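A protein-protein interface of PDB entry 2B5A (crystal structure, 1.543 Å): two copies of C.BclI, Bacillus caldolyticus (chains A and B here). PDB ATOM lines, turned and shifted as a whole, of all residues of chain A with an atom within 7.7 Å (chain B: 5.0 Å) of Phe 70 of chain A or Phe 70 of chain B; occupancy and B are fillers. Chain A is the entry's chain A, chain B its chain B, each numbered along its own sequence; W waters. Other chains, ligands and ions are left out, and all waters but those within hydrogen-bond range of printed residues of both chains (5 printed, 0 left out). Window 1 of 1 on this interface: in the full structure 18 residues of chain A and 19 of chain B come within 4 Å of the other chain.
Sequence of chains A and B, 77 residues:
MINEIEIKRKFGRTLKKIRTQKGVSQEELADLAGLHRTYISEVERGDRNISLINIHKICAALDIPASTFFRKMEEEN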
ATOM      1  N   ILE A   7     -22.950 -27.914 -33.749  1.00  0.00           N
ATOM      2  CA  ILE A   7     -23.236 -26.593 -33.209  1.00  0.00           C
ATOM      3  C   ILE A   7     -23.996 -26.736 -31.886  1.00  0.00           C
ATOM      4  O   ILE A   7     -23.659 -26.116 -30.892  1.00  0.00           O
ATOM      5  CB  ILE A   7     -24.022 -25.732 -34.195  1.00  0.00           C
ATOM      6  CG1 ILE A   7     -23.150 -25.391 -35.398  1.00  0.00           C
ATOM      7  CG2 ILE A   7     -24.590 -24.457 -33.545  1.00  0.00           C
ATOM      8  CD1 ILE A   7     -23.962 -24.940 -36.592  1.00  0.00           C
ATOM      9  N   LYS A  10     -21.789 -28.391 -29.188  1.00  0.00           N
ATOM     10  CA  LYS A  10     -20.780 -27.443 -28.689  1.00  0.00           C
ATOM     11  C   LYS A  10     -21.384 -26.452 -27.691  1.00  0.00           C
ATOM     12  O   LYS A  10     -20.792 -26.162 -26.634  1.00  0.00           O
ATOM     13  CB  LYS A  10     -20.151 -26.675 -29.835  1.00  0.00           C
ATOM     14  CG  LYS A  10     -19.007 -25.798 -29.389  1.00  0.00           C
ATOM     15  CD  LYS A  10     -18.433 -25.023 -30.558  1.00  0.00           C
ATOM     16  CE  LYS A  10     -17.592 -25.908 -31.438  1.00  0.00           C
ATOM     17  NZ  LYS A  10     -16.739 -25.111 -32.375  1.00  0.00           N
ATOM     18  N   PHE A  11     -22.583 -25.947 -28.000  1.00  0.00           N
ATOM     19  CA  PHE A  11     -23.282 -25.096 -27.067  1.00  0.00           C
ATOM     20  C   PHE A  11     -23.484 -25.833 -25.736  1.00  0.00           C
ATOM     21  O   PHE A  11     -23.266 -25.299 -24.651  1.00  0.00           O
ATOM     22  CB  PHE A  11     -24.629 -24.627 -27.614  1.00  0.00           C
ATOM     23  CG  PHE A  11     -25.348 -23.705 -26.694  1.00  0.00           C
ATOM     24  CD1 PHE A  11     -25.247 -22.342 -26.834  1.00  0.00           C
ATOM     25  CD2 PHE A  11     -26.137 -24.212 -25.678  1.00  0.00           C
ATOM     26  CE1 PHE A  11     -25.889 -21.506 -25.932  1.00  0.00           C
ATOM     27  CE2 PHE A  11     -26.802 -23.402 -24.804  1.00  0.00           C
ATOM     28  CZ  PHE A  11     -26.670 -22.027 -24.924  1.00  0.00           C
ATOM     29  N   THR A  14     -20.314 -26.328 -23.682  1.00  0.00           N
ATOM     30  CA  THR A  14     -19.907 -25.065 -23.105  1.00  0.00           C
ATOM     31  C   THR A  14     -20.788 -24.728 -21.896  1.00  0.00           C
ATOM     32  O   THR A  14     -20.309 -24.273 -20.871  1.00  0.00           O
ATOM     33  CB  THR A  14     -19.975 -23.967 -24.153  1.00  0.00           C
ATOM     34  OG1 THR A  14     -19.129 -24.299 -25.283  1.00  0.00           O
ATOM     35  CG2 THR A  14     -19.532 -22.633 -23.575  1.00  0.00           C
ATOM     36  N   ILE A  18     -19.389 -24.205 -18.077  1.00  0.00           N
ATOM     37  CA  ILE A  18     -19.597 -22.972 -17.347  1.00  0.00           C
ATOM     38  C   ILE A  18     -20.428 -23.218 -16.091  1.00  0.00           C
ATOM     39  O   ILE A  18     -20.104 -22.711 -15.013  1.00  0.00           O
ATOM     40  CB  ILE A  18     -20.261 -21.901 -18.235  1.00  0.00           C
ATOM     41  CG1 ILE A  18     -19.321 -21.530 -19.395  1.00  0.00           C
ATOM     42  CG2 ILE A  18     -20.614 -20.656 -17.395  1.00  0.00           C
ATOM     43  CD1 ILE A  18     -19.891 -20.610 -20.423  1.00  0.00           C
ATOM     44  N   ILE A  50     -32.112 -25.087 -29.081  1.00  0.00           N
ATOM     45  CA  ILE A  50     -32.089 -23.933 -28.202  1.00  0.00           C
ATOM     46  C   ILE A  50     -32.071 -22.694 -29.052  1.00  0.00           C
ATOM     47  O   ILE A  50     -31.443 -22.646 -30.142  1.00  0.00           O
ATOM     48  CB  ILE A  50     -31.011 -23.867 -27.048  1.00  0.00           C
ATOM     49  CG1 ILE A  50     -31.520 -22.904 -25.941  1.00  0.00           C
ATOM     50  CG2 ILE A  50     -29.695 -23.371 -27.490  1.00  0.00           C
ATOM     51  CD1 ILE A  50     -30.672 -22.834 -24.766  1.00  0.00           C
ATOM     52  N   LEU A  52     -32.877 -18.125 -28.990  1.00  0.00           N
ATOM     53  CA  LEU A  52     -32.446 -16.871 -28.375  1.00  0.00           C
ATOM     54  C   LEU A  52     -32.944 -16.663 -26.946  1.00  0.00           C
ATOM     55  O   LEU A  52     -32.175 -16.340 -26.035  1.00  0.00           O
ATOM     56  CB  LEU A  52     -32.932 -15.701 -29.227  1.00  0.00           C
ATOM     57  CG  LEU A  52     -32.540 -14.295 -28.787  1.00  0.00           C
ATOM     58  CD1 LEU A  52     -31.072 -14.081 -29.023  1.00  0.00           C
ATOM     59  CD2 LEU A  52     -33.326 -13.247 -29.538  1.00  0.00           C
ATOM     60  N   ILE A  55     -31.431 -19.183 -24.480  1.00  0.00           N
ATOM     61  CA  ILE A  55     -30.018 -18.823 -24.344  1.00  0.00           C
ATOM     62  C   ILE A  55     -29.880 -17.704 -23.334  1.00  0.00           C
ATOM     63  O   ILE A  55     -29.055 -17.783 -22.430  1.00  0.00           O
ATOM     64  CB  ILE A  55     -29.378 -18.424 -25.706  1.00  0.00           C
ATOM     65  CG1 ILE A  55     -29.305 -19.636 -26.638  1.00  0.00           C
ATOM     66  CG2 ILE A  55     -27.990 -17.774 -25.481  1.00  0.00           C
ATOM     67  CD1 ILE A  55     -28.969 -19.296 -28.091  1.00  0.00           C
ATOM     68  N   HIS A  56     -30.664 -16.645 -23.486  1.00  0.00           N
ATOM     69  CA  HIS A  56     -30.579 -15.532 -22.542  1.00  0.00           C
ATOM     70  C   HIS A  56     -31.068 -15.836 -21.135  1.00  0.00           C
ATOM     71  O   HIS A  56     -30.479 -15.358 -20.181  1.00  0.00           O
ATOM     72  CB  HIS A  56     -31.223 -14.305 -23.151  1.00  0.00           C
ATOM     73  CG  HIS A  56     -30.350 -13.693 -24.190  1.00  0.00           C
ATOM     74  ND1 HIS A  56     -30.223 -14.211 -25.462  1.00  0.00           N
ATOM     75  CD2 HIS A  56     -29.466 -12.670 -24.104  1.00  0.00           C
ATOM     76  CE1 HIS A  56     -29.327 -13.497 -26.130  1.00  0.00           C
ATOM     77  NE2 HIS A  56     -28.861 -12.554 -25.330  1.00  0.00           N
ATOM     78  N   CYS A  59     -28.092 -17.769 -19.616  1.00  0.00           N
ATOM     79  CA  CYS A  59     -26.950 -16.897 -19.343  1.00  0.00           C
ATOM     80  C   CYS A  59     -27.237 -15.944 -18.173  1.00  0.00           C
ATOM     81  O   CYS A  59     -26.369 -15.703 -17.347  1.00  0.00           O
ATOM     82  CB  CYS A  59     -26.560 -16.103 -20.583  1.00  0.00           C
ATOM     83  SG  CYS A  59     -25.706 -17.078 -21.853  1.00  0.00           S
ATOM     84  N   ILE A  64     -23.754 -14.455 -16.553  1.00  0.00           N
ATOM     85  CA  ILE A  64     -22.722 -14.298 -17.572  1.00  0.00           C
ATOM     86  C   ILE A  64     -23.394 -13.627 -18.784  1.00  0.00           C
ATOM     87  O   ILE A  64     -24.524 -13.971 -19.145  1.00  0.00           O
ATOM     88  CB  ILE A  64     -22.109 -15.669 -17.952  1.00  0.00           C
ATOM     89  CG1 ILE A  64     -20.858 -15.553 -18.844  1.00  0.00           C
ATOM     90  CG2 ILE A  64     -23.139 -16.587 -18.609  1.00  0.00           C
ATOM     91  CD1 ILE A  64     -20.167 -16.933 -19.139  1.00  0.00           C
ATOM     92  N   PRO A  65     -22.715 -12.660 -19.400  1.00  0.00           N
ATOM     93  CA  PRO A  65     -23.242 -12.111 -20.657  1.00  0.00           C
ATOM     94  C   PRO A  65     -23.234 -13.159 -21.766  1.00  0.00           C
ATOM     95  O   PRO A  65     -22.326 -13.990 -21.817  1.00  0.00           O
ATOM     96  CB  PRO A  65     -22.266 -10.963 -20.981  1.00  0.00           C
ATOM     97  CG  PRO A  65     -21.489 -10.741 -19.761  1.00  0.00           C
ATOM     98  CD  PRO A  65     -21.453 -12.014 -19.000  1.00  0.00           C
ATOM     99  N   ALA A  66     -24.236 -13.122 -22.652  1.00  0.00           N
ATOM    100  CA  ALA A  66     -24.245 -14.038 -23.799  1.00  0.00           C
ATOM    101  C   ALA A  66     -22.958 -13.908 -24.602  1.00  0.00           C
ATOM    102  O   ALA A  66     -22.416 -14.910 -25.065  1.00  0.00           O
ATOM    103  CB  ALA A  66     -25.469 -13.852 -24.676  1.00  0.00           C
ATOM    104  N   SER A  67     -22.440 -12.690 -24.764  1.00  0.00           N
ATOM    105  CA  SER A  67     -21.194 -12.520 -25.508  1.00  0.00           C
ATOM    106  C   SER A  67     -20.067 -13.357 -24.910  1.00  0.00           C
ATOM    107  O   SER A  67     -19.284 -13.932 -25.630  1.00  0.00           O
ATOM    108  CB  SER A  67     -20.775 -11.052 -25.568  1.00  0.00           C
ATOM    109  OG  SER A  67     -20.661 -10.484 -24.272  1.00  0.00           O
ATOM    110  N   THR A  68     -19.987 -13.416 -23.576  1.00  0.00           N
ATOM    111  CA  THR A  68     -18.927 -14.165 -22.926  1.00  0.00           C
ATOM    112  C   THR A  68     -19.144 -15.663 -23.096  1.00  0.00           C
ATOM    113  O   THR A  68     -18.189 -16.417 -23.305  1.00  0.00           O
ATOM    114  CB  THR A  68     -18.883 -13.809 -21.455  1.00  0.00           C
ATOM    115  OG1 THR A  68     -18.595 -12.415 -21.323  1.00  0.00           O
ATOM    116  CG2 THR A  68     -17.812 -14.611 -20.721  1.00  0.00           C
ATOM    117  N   PHE A  69     -20.397 -16.083 -23.021  1.00  0.00           N
ATOM    118  CA  PHE A  69     -20.752 -17.484 -23.277  1.00  0.00           C
ATOM    119  C   PHE A  69     -20.261 -17.857 -24.666  1.00  0.00           C
ATOM    120  O   PHE A  69     -19.556 -18.843 -24.854  1.00  0.00           O
ATOM    121  CB  PHE A  69     -22.265 -17.730 -23.156  1.00  0.00           C
ATOM    122  CG  PHE A  69     -22.645 -19.179 -23.286  1.00  0.00           C
ATOM    123  CD1 PHE A  69     -22.991 -19.939 -22.178  1.00  0.00           C
ATOM    124  CD2 PHE A  69     -22.643 -19.797 -24.516  1.00  0.00           C
ATOM    125  CE1 PHE A  69     -23.333 -21.305 -22.342  1.00  0.00           C
ATOM    126  CE2 PHE A  69     -22.969 -21.138 -24.659  1.00  0.00           C
ATOM    127  CZ  PHE A  69     -23.311 -21.877 -23.566  1.00  0.00           C
ATOM    128  N   PHE A  70     -20.591 -17.045 -25.665  1.00  0.00           N
ATOM    129  CA  PHE A  70     -20.251 -17.400 -27.043  1.00  0.00           C
ATOM    130  C   PHE A  70     -18.751 -17.283 -27.292  1.00  0.00           C
ATOM    131  O   PHE A  70     -18.197 -18.009 -28.099  1.00  0.00           O
ATOM    132  CB  PHE A  70     -21.066 -16.581 -28.034  1.00  0.00           C
ATOM    133  CG  PHE A  70     -22.439 -17.145 -28.236  1.00  0.00           C
ATOM    134  CD1 PHE A  70     -22.665 -18.086 -29.194  1.00  0.00           C
ATOM    135  CD2 PHE A  70     -23.468 -16.800 -27.398  1.00  0.00           C
ATOM    136  CE1 PHE A  70     -23.918 -18.643 -29.377  1.00  0.00           C
ATOM    137  CE2 PHE A  70     -24.735 -17.374 -27.559  1.00  0.00           C
ATOM    138  CZ  PHE A  70     -24.942 -18.290 -28.567  1.00  0.00           C
ATOM    139  N   ARG A  71     -18.080 -16.367 -26.602  1.00  0.00           N
ATOM    140  CA  ARG A  71     -16.636 -16.280 -26.717  1.00  0.00           C
ATOM    141  C   ARG A  71     -15.995 -17.580 -26.220  1.00  0.00           C
ATOM    142  O   ARG A  71     -15.082 -18.104 -26.855  1.00  0.00           O
ATOM    143  CB  ARG A  71     -16.086 -15.065 -25.965  1.00  0.00           C
ATOM    144  CG  ARG A  71     -14.602 -14.817 -26.218  1.00  0.00           C
ATOM    145  CD  ARG A  71     -13.934 -14.033 -25.085  1.00  0.00           C
ATOM    146  NE  ARG A  71     -13.833 -14.830 -23.853  1.00  0.00           N
ATOM    147  CZ  ARG A  71     -14.157 -14.420 -22.624  1.00  0.00           C
ATOM    148  NH1 ARG A  71     -14.601 -13.190 -22.391  1.00  0.00           N
ATOM    149  NH2 ARG A  71     -14.024 -15.259 -21.604  1.00  0.00           N
ATOM    150  N   LYS A  72     -16.481 -18.102 -25.101  1.00  0.00           N
ATOM    151  CA  LYS A  72     -15.978 -19.383 -24.605  1.00  0.00           C
ATOM    152  C   LYS A  72     -16.280 -20.534 -25.579  1.00  0.00           C
ATOM    153  O   LYS A  72     -15.437 -21.408 -25.830  1.00  0.00           O
ATOM    154  CB  LYS A  72     -16.561 -19.663 -23.226  1.00  0.00           C
ATOM    155  CG  LYS A  72     -16.019 -18.748 -22.166  1.00  0.00           C
ATOM    156  CD  LYS A  72     -16.712 -18.941 -20.824  1.00  0.00           C
ATOM    157  CE  LYS A  72     -16.067 -18.101 -19.740  1.00  0.00           C
ATOM    158  NZ  LYS A  72     -14.697 -18.586 -19.382  1.00  0.00           N
ATOM    159  N   MET A  73     -17.468 -20.518 -26.164  1.00  0.00           N
ATOM    160  CA  MET A  73     -17.820 -21.507 -27.165  1.00  0.00           C
ATOM    161  C   MET A  73     -16.833 -21.448 -28.342  1.00  0.00           C
ATOM    162  O   MET A  73     -16.387 -22.474 -28.856  1.00  0.00           O
ATOM    163  CB  MET A  73     -19.264 -21.298 -27.627  1.00  0.00           C
ATOM    164  CG  MET A  73     -19.885 -22.463 -28.338  1.00  0.00           C
ATOM    165  SD  MET A  73     -21.601 -22.090 -28.710  1.00  0.00           S
ATOM    166  CE  MET A  73     -21.932 -23.228 -30.074  1.00  0.00           C
ATOM    167  N   GLU A  74     -16.512 -20.239 -28.770  1.00  0.00           N
ATOM    168  CA  GLU A  74     -15.613 -20.004 -29.894  1.00  0.00           C
ATOM    169  C   GLU A  74     -14.168 -20.434 -29.610  1.00  0.00           C
ATOM    170  O   GLU A  74     -13.439 -20.804 -30.537  1.00  0.00           O
ATOM    171  CB  GLU A  74     -15.665 -18.520 -30.279  1.00  0.00           C
ATOM    172  CG  GLU A  74     -16.979 -18.105 -30.916  1.00  0.00           C
ATOM    173  CD  GLU A  74     -17.272 -16.588 -30.866  1.00  0.00           C
ATOM    174  OE1 GLU A  74     -16.392 -15.772 -30.516  1.00  0.00           O
ATOM    175  OE2 GLU A  74     -18.432 -16.239 -31.182  1.00  0.00           O
ATOM    176  N   GLU A  75     -13.785 -20.366 -28.335  1.00  0.00           N
ATOM    177  CA  GLU A  75     -12.416 -20.659 -27.896  1.00  0.00           C
ATOM    178  C   GLU A  75     -12.204 -22.140 -27.670  1.00  0.00           C
ATOM    179  O   GLU A  75     -11.063 -22.567 -27.443  1.00  0.00           O
ATOM    180  CB  GLU A  75     -12.104 -19.921 -26.589  1.00  0.00           C
ATOM    181  CG  GLU A  75     -11.933 -18.414 -26.740  1.00  0.00           C
ATOM    182  CD  GLU A  75     -11.882 -17.677 -25.399  1.00  0.00           C
ATOM    183  OE1 GLU A  75     -11.994 -18.327 -24.331  1.00  0.00           O
ATOM    184  OE2 GLU A  75     -11.735 -16.433 -25.419  1.00  0.00           O
ATOM    185  N   GLU A  76     -13.275 -22.926 -27.706  1.00  0.00           N
ATOM    186  CA  GLU A  76     -13.158 -24.376 -27.532  1.00  0.00           C
ATOM    187  C   GLU A  76     -12.374 -24.989 -28.682  1.00  0.00           C
ATOM    188  O   GLU A  76     -12.658 -24.699 -29.846  1.00  0.00           O
ATOM    189  CB  GLU A  76     -14.530 -25.042 -27.486  1.00  0.00           C
ATOM    190  CG  GLU A  76     -14.505 -26.440 -26.866  1.00  0.00           C
ATOM    191  CD  GLU A  76     -15.689 -27.300 -27.262  1.00  0.00           C
ATOM    192  OE1 GLU A  76     -15.962 -27.389 -28.474  1.00  0.00           O
ATOM    193  OE2 GLU A  76     -16.333 -27.895 -26.366  1.00  0.00           O
ATOM    194  N   PHE B  11     -32.211  -7.973 -30.232  1.00  0.00           N
ATOM    195  CA  PHE B  11     -31.461  -8.784 -31.196  1.00  0.00           C
ATOM    196  C   PHE B  11     -31.787  -8.312 -32.618  1.00  0.00           C
ATOM    197  O   PHE B  11     -30.898  -8.150 -33.446  1.00  0.00           O
ATOM    198  CB  PHE B  11     -31.831 -10.263 -31.071  1.00  0.00           C
ATOM    199  CG  PHE B  11     -31.102 -11.145 -32.042  1.00  0.00           C
ATOM    200  CD1 PHE B  11     -29.891 -11.726 -31.709  1.00  0.00           C
ATOM    201  CD2 PHE B  11     -31.611 -11.349 -33.316  1.00  0.00           C
ATOM    202  CE1 PHE B  11     -29.197 -12.525 -32.636  1.00  0.00           C
ATOM    203  CE2 PHE B  11     -30.933 -12.102 -34.241  1.00  0.00           C
ATOM    204  CZ  PHE B  11     -29.720 -12.707 -33.896  1.00  0.00           C
ATOM    205  N   LEU B  52     -30.405 -21.039 -32.231  1.00  0.00           N
ATOM    206  CA  LEU B  52     -28.939 -21.086 -32.244  1.00  0.00           C
ATOM    207  C   LEU B  52     -28.386 -21.317 -33.649  1.00  0.00           C
ATOM    208  O   LEU B  52     -27.462 -20.622 -34.080  1.00  0.00           O
ATOM    209  CB  LEU B  52     -28.459 -22.177 -31.316  1.00  0.00           C
ATOM    210  CG  LEU B  52     -26.948 -22.405 -31.298  1.00  0.00           C
ATOM    211  CD1 LEU B  52     -26.212 -21.186 -30.767  1.00  0.00           C
ATOM    212  CD2 LEU B  52     -26.629 -23.656 -30.452  1.00  0.00           C
ATOM    213  N   ILE B  55     -28.796 -18.159 -35.706  1.00  0.00           N
ATOM    214  CA  ILE B  55     -27.817 -17.184 -35.202  1.00  0.00           C
ATOM    215  C   ILE B  55     -26.453 -17.466 -35.835  1.00  0.00           C
ATOM    216  O   ILE B  55     -25.811 -16.569 -36.366  1.00  0.00           O
ATOM    217  CB  ILE B  55     -27.711 -17.204 -33.655  1.00  0.00           C
ATOM    218  CG1 ILE B  55     -29.026 -16.673 -33.042  1.00  0.00           C
ATOM    219  CG2 ILE B  55     -26.527 -16.384 -33.167  1.00  0.00           C
ATOM    220  CD1 ILE B  55     -29.149 -16.951 -31.564  1.00  0.00           C
ATOM    221  N   ALA B  66     -20.304 -14.558 -33.258  1.00  0.00           N
ATOM    222  CA  ALA B  66     -21.478 -14.407 -32.400  1.00  0.00           C
ATOM    223  C   ALA B  66     -21.151 -13.641 -31.133  1.00  0.00           C
ATOM    224  O   ALA B  66     -21.971 -12.834 -30.670  1.00  0.00           O
ATOM    225  CB  ALA B  66     -22.076 -15.781 -32.038  1.00  0.00           C
ATOM    226  N   SER B  67     -19.964 -13.870 -30.562  1.00  0.00           N
ATOM    227  CA  SER B  67     -19.590 -13.148 -29.331  1.00  0.00           C
ATOM    228  C   SER B  67     -19.589 -11.645 -29.571  1.00  0.00           C
ATOM    229  O   SER B  67     -20.112 -10.888 -28.765  1.00  0.00           O
ATOM    230  CB  SER B  67     -18.217 -13.585 -28.846  1.00  0.00           C
ATOM    231  OG  SER B  67     -17.233 -13.442 -29.854  1.00  0.00           O
ATOM    232  N   THR B  68     -19.050 -11.231 -30.693  1.00  0.00           N
ATOM    233  CA  THR B  68     -18.993  -9.807 -31.046  1.00  0.00           C
ATOM    234  C   THR B  68     -20.396  -9.259 -31.323  1.00  0.00           C
ATOM    235  O   THR B  68     -20.722  -8.131 -30.934  1.00  0.00           O
ATOM    236  CB  THR B  68     -18.122  -9.613 -32.294  1.00  0.00           C
ATOM    237  OG1 THR B  68     -16.832 -10.195 -32.066  1.00  0.00           O
ATOM    238  CG2 THR B  68     -17.989  -8.107 -32.642  1.00  0.00           C
ATOM    239  N   PHE B  69     -21.219 -10.019 -32.034  1.00  0.00           N
ATOM    240  CA  PHE B  69     -22.609  -9.642 -32.268  1.00  0.00           C
ATOM    241  C   PHE B  69     -23.277  -9.392 -30.919  1.00  0.00           C
ATOM    242  O   PHE B  69     -23.909  -8.372 -30.700  1.00  0.00           O
ATOM    243  CB  PHE B  69     -23.359 -10.749 -33.015  1.00  0.00           C
ATOM    244  CG  PHE B  69     -24.789 -10.389 -33.360  1.00  0.00           C
ATOM    245  CD1 PHE B  69     -25.128 -10.045 -34.668  1.00  0.00           C
ATOM    246  CD2 PHE B  69     -25.778 -10.403 -32.398  1.00  0.00           C
ATOM    247  CE1 PHE B  69     -26.459  -9.746 -34.979  1.00  0.00           C
ATOM    248  CE2 PHE B  69     -27.104 -10.042 -32.712  1.00  0.00           C
ATOM    249  CZ  PHE B  69     -27.405  -9.710 -34.005  1.00  0.00           C
ATOM    250  N   PHE B  70     -23.167 -10.330 -30.002  1.00  0.00           N
ATOM    251  CA  PHE B  70     -23.847 -10.152 -28.720  1.00  0.00           C
ATOM    252  C   PHE B  70     -23.253  -9.019 -27.892  1.00  0.00           C
ATOM    253  O   PHE B  70     -23.990  -8.386 -27.129  1.00  0.00           O
ATOM    254  CB  PHE B  70     -23.920 -11.461 -27.935  1.00  0.00           C
ATOM    255  CG  PHE B  70     -24.939 -12.406 -28.467  1.00  0.00           C
ATOM    256  CD1 PHE B  70     -26.270 -12.082 -28.470  1.00  0.00           C
ATOM    257  CD2 PHE B  70     -24.549 -13.628 -29.009  1.00  0.00           C
ATOM    258  CE1 PHE B  70     -27.220 -12.949 -28.989  1.00  0.00           C
ATOM    259  CE2 PHE B  70     -25.500 -14.510 -29.531  1.00  0.00           C
ATOM    260  CZ  PHE B  70     -26.827 -14.142 -29.530  1.00  0.00           C
ATOM    261  N   ARG B  71     -21.955  -8.750 -28.022  1.00  0.00           N
ATOM    262  CA  ARG B  71     -21.357  -7.607 -27.332  1.00  0.00           C
ATOM    263  C   ARG B  71     -22.032  -6.324 -27.820  1.00  0.00           C
ATOM    264  O   ARG B  71     -22.350  -5.447 -27.024  1.00  0.00           O
ATOM    265  CB  ARG B  71     -19.855  -7.580 -27.548  1.00  0.00           C
ATOM    266  CG  ARG B  71     -19.120  -6.642 -26.610  1.00  0.00           C
ATOM    267  CD  ARG B  71     -17.605  -6.869 -26.673  1.00  0.00           C
ATOM    268  NE  ARG B  71     -17.258  -8.261 -26.370  1.00  0.00           N
ATOM    269  CZ  ARG B  71     -16.692  -9.137 -27.207  1.00  0.00           C
ATOM    270  NH1 ARG B  71     -16.346  -8.791 -28.450  1.00  0.00           N
ATOM    271  NH2 ARG B  71     -16.448 -10.378 -26.778  1.00  0.00           N
ATOM    272  N   LYS B  72     -22.262  -6.225 -29.129  1.00  0.00           N
ATOM    273  CA  LYS B  72     -22.962  -5.045 -29.690  1.00  0.00           C
ATOM    274  C   LYS B  72     -24.408  -4.961 -29.170  1.00  0.00           C
ATOM    275  O   LYS B  72     -24.896  -3.882 -28.799  1.00  0.00           O
ATOM    276  CB  LYS B  72     -22.899  -5.060 -31.221  1.00  0.00           C
ATOM    277  CG  LYS B  72     -21.488  -4.894 -31.730  1.00  0.00           C
ATOM    278  CD  LYS B  72     -21.410  -5.139 -33.230  1.00  0.00           C
ATOM    279  CE  LYS B  72     -20.019  -4.846 -33.794  1.00  0.00           C
ATOM    280  NZ  LYS B  72     -19.607  -3.415 -33.684  1.00  0.00           N
ATOM    281  N   MET B  73     -25.083  -6.100 -29.109  1.00  0.00           N
ATOM    282  CA  MET B  73     -26.458  -6.171 -28.606  1.00  0.00           C
ATOM    283  C   MET B  73     -26.519  -5.726 -27.146  1.00  0.00           C
ATOM    284  O   MET B  73     -27.521  -5.124 -26.711  1.00  0.00           O
ATOM    285  CB  MET B  73     -26.986  -7.597 -28.710  1.00  0.00           C
ATOM    286  CG  MET B  73     -28.454  -7.764 -28.373  1.00  0.00           C
ATOM    287  SD  MET B  73     -28.955  -9.468 -28.525  1.00  0.00           S
ATOM    288  CE  MET B  73     -30.235  -9.621 -27.267  1.00  0.00           C
ATOM    289  N   GLU B  74     -25.461  -6.032 -26.401  1.00  0.00           N
ATOM    290  CA  GLU B  74     -25.382  -5.724 -24.982  1.00  0.00           C
ATOM    291  C   GLU B  74     -25.075  -4.252 -24.683  1.00  0.00           C
ATOM    292  O   GLU B  74     -25.314  -3.806 -23.547  1.00  0.00           O
ATOM    293  CB  GLU B  74     -24.360  -6.636 -24.301  1.00  0.00           C
ATOM    294  CG  GLU B  74     -24.824  -8.072 -24.279  1.00  0.00           C
ATOM    295  CD  GLU B  74     -23.706  -9.114 -24.211  1.00  0.00           C
ATOM    296  OE1 GLU B  74     -22.522  -8.779 -24.001  1.00  0.00           O
ATOM    297  OE2 GLU B  74     -24.083 -10.285 -24.412  1.00  0.00           O
HETATM  298  O   HOH W   1     -30.841 -24.229 -32.681  1.00  0.00           O
HETATM  299  O   HOH W   2     -16.119 -11.419 -23.859  1.00  0.00           O
HETATM  300  O   HOH W   3     -27.003 -10.540 -24.862  1.00  0.00           O
HETATM  301  O   HOH W   4     -19.397 -17.278 -33.764  1.00  0.00           O
HETATM  302  O   HOH W   5     -26.476 -11.315 -22.082  1.00  0.00           O
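The backbone carbonyl oxygen of Ile 50 of chain A is in hydrogen-bond range of the backbone NH of Leu 52 of chain B (2.8 Å). The backbone NH of Ala 66 of chain A is in hydrogen-bond range of the side-chain carboxylate of Glu 74 of chain B. OG of Ser 67 of chain A sits at hydrogen-bond distance from OE1 of Glu 74 of chain B, 2.5 Å away. The side-chain carboxylate of Glu 74 of chain A lies within hydrogen-bond range of the backbone NH of Ala 66 of chain B, 3.3 Å away. The side-chain hydroxyl of Ser 67 of chain B lies within hydrogen-bond range of the side-chain carboxylate of Glu 74 of chain A (2.6 Å).
O of Leu 52 of chain A is in hydrogen-bond range of ND1 of His 56 of chain A, at 2.9 Å. NE of Arg 71 of chain A is in salt-bridge range of OE2 of Glu 75 of chain A.
Among the printed residues, pairs that only touch across the chains: Ser 67 of chain A with Ser 67 of chain B (3.3 Å), Phe 70 of chain A with Phe 70 of chain B (3.6 Å), Ser 67 of chain A with Arg 71 of chain B (3.6 Å), Arg 71 of chain A with Ser 67 of chain B (3.6 Å), His 56 of chain A with Phe 70 of chain B (3.6 Å), Phe 11 of chain A with Leu 52 of chain B (3.6 Å), Leu 52 of chain A with Phe 11 of chain B (3.7 Å), Phe 70 of chain A with Leu 52 of chain B (3.7 Å), Phe 70 of chain A with Ala 66 of chain B (3.7 Å), Ser 67 of chain A with Phe 70 of chain B (3.7 Å), Pro 65 of chain A with Glu 74 of chain B (3.7 Å), His 56 of chain A with Met 73 of chain B (3.8 Å), Ile 7 of chain A with Leu 52 of chain B (3.8 Å) and Phe 70 of chain A with Ser 67 of chain B (3.9 Å).
Thr 14 of chain A touches none of the printed residues of chain B. Printed residues of chain B within 4 Å of His 56 of chain A: Phe 70 and Met 73. Of the printed residues of chain B, Pro 65 of chain A touches Glu 74. Phe 70 of chain A touches just these residues of chain B: Leu 52, Ala 66, Ser 67 and Phe 70. Of the printed residues of chain A, Arg 71 of chain B touches Ser 67. The nearest printed residue of chain B that does not touch Phe 70 of chain A is Ile 55 of chain B (5.1 Å).
Of the 23 printed residues of chain A, 11 touch a printed residue of chain B. Hydrophobic or aromatic side chains of chain A within 4 Å of the printed part of chain B: Ile 7, Phe 11, Leu 52, His 56, Pro 65, Ala 66 and Phe 70. Of the 12 printed residues of chain B, 8 touch a printed residue of chain A. Along chain B the printed residues that touch a printed residue of chain A span positions 11 to 74. Among the printed residues, 19 pairs touch across the chains. Among the printed residues, no Asp or Glu carboxylate lies within 4 Å of a Lys or Arg side-chain nitrogen of the other chain.
Ser 67 of chain A touches Phe 70 of chain B, and with the chains exchanged Phe 70 of chain A touches Ser 67 of chain B. Ser 67 of chain A touches Glu 74 of chain B, and with the chains exchanged Glu 74 of chain A touches Ser 67 of chain B. Positions printed for both chains: 11, 52, 55, 66, 67, 68, 69, 70, 71, 72, 73 and 74.
Water W2 bridges NH1 of Arg 71 of chain A (2.8 Å) and NH2 of Arg 71 of chain B (3.1 Å). Water W3 bridges a ring nitrogen (NE2) of His 56 of chain A (2.8 Å) and the side-chain carboxylate (OE2) of Glu 74 of chain B (3.0 Å). Water W1 lies within hydrogen-bond range of the backbone carbonyl oxygen of Ile 50 of chain A (3.1 Å) and the backbone NH of Leu 52 of chain B (3.3 Å).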
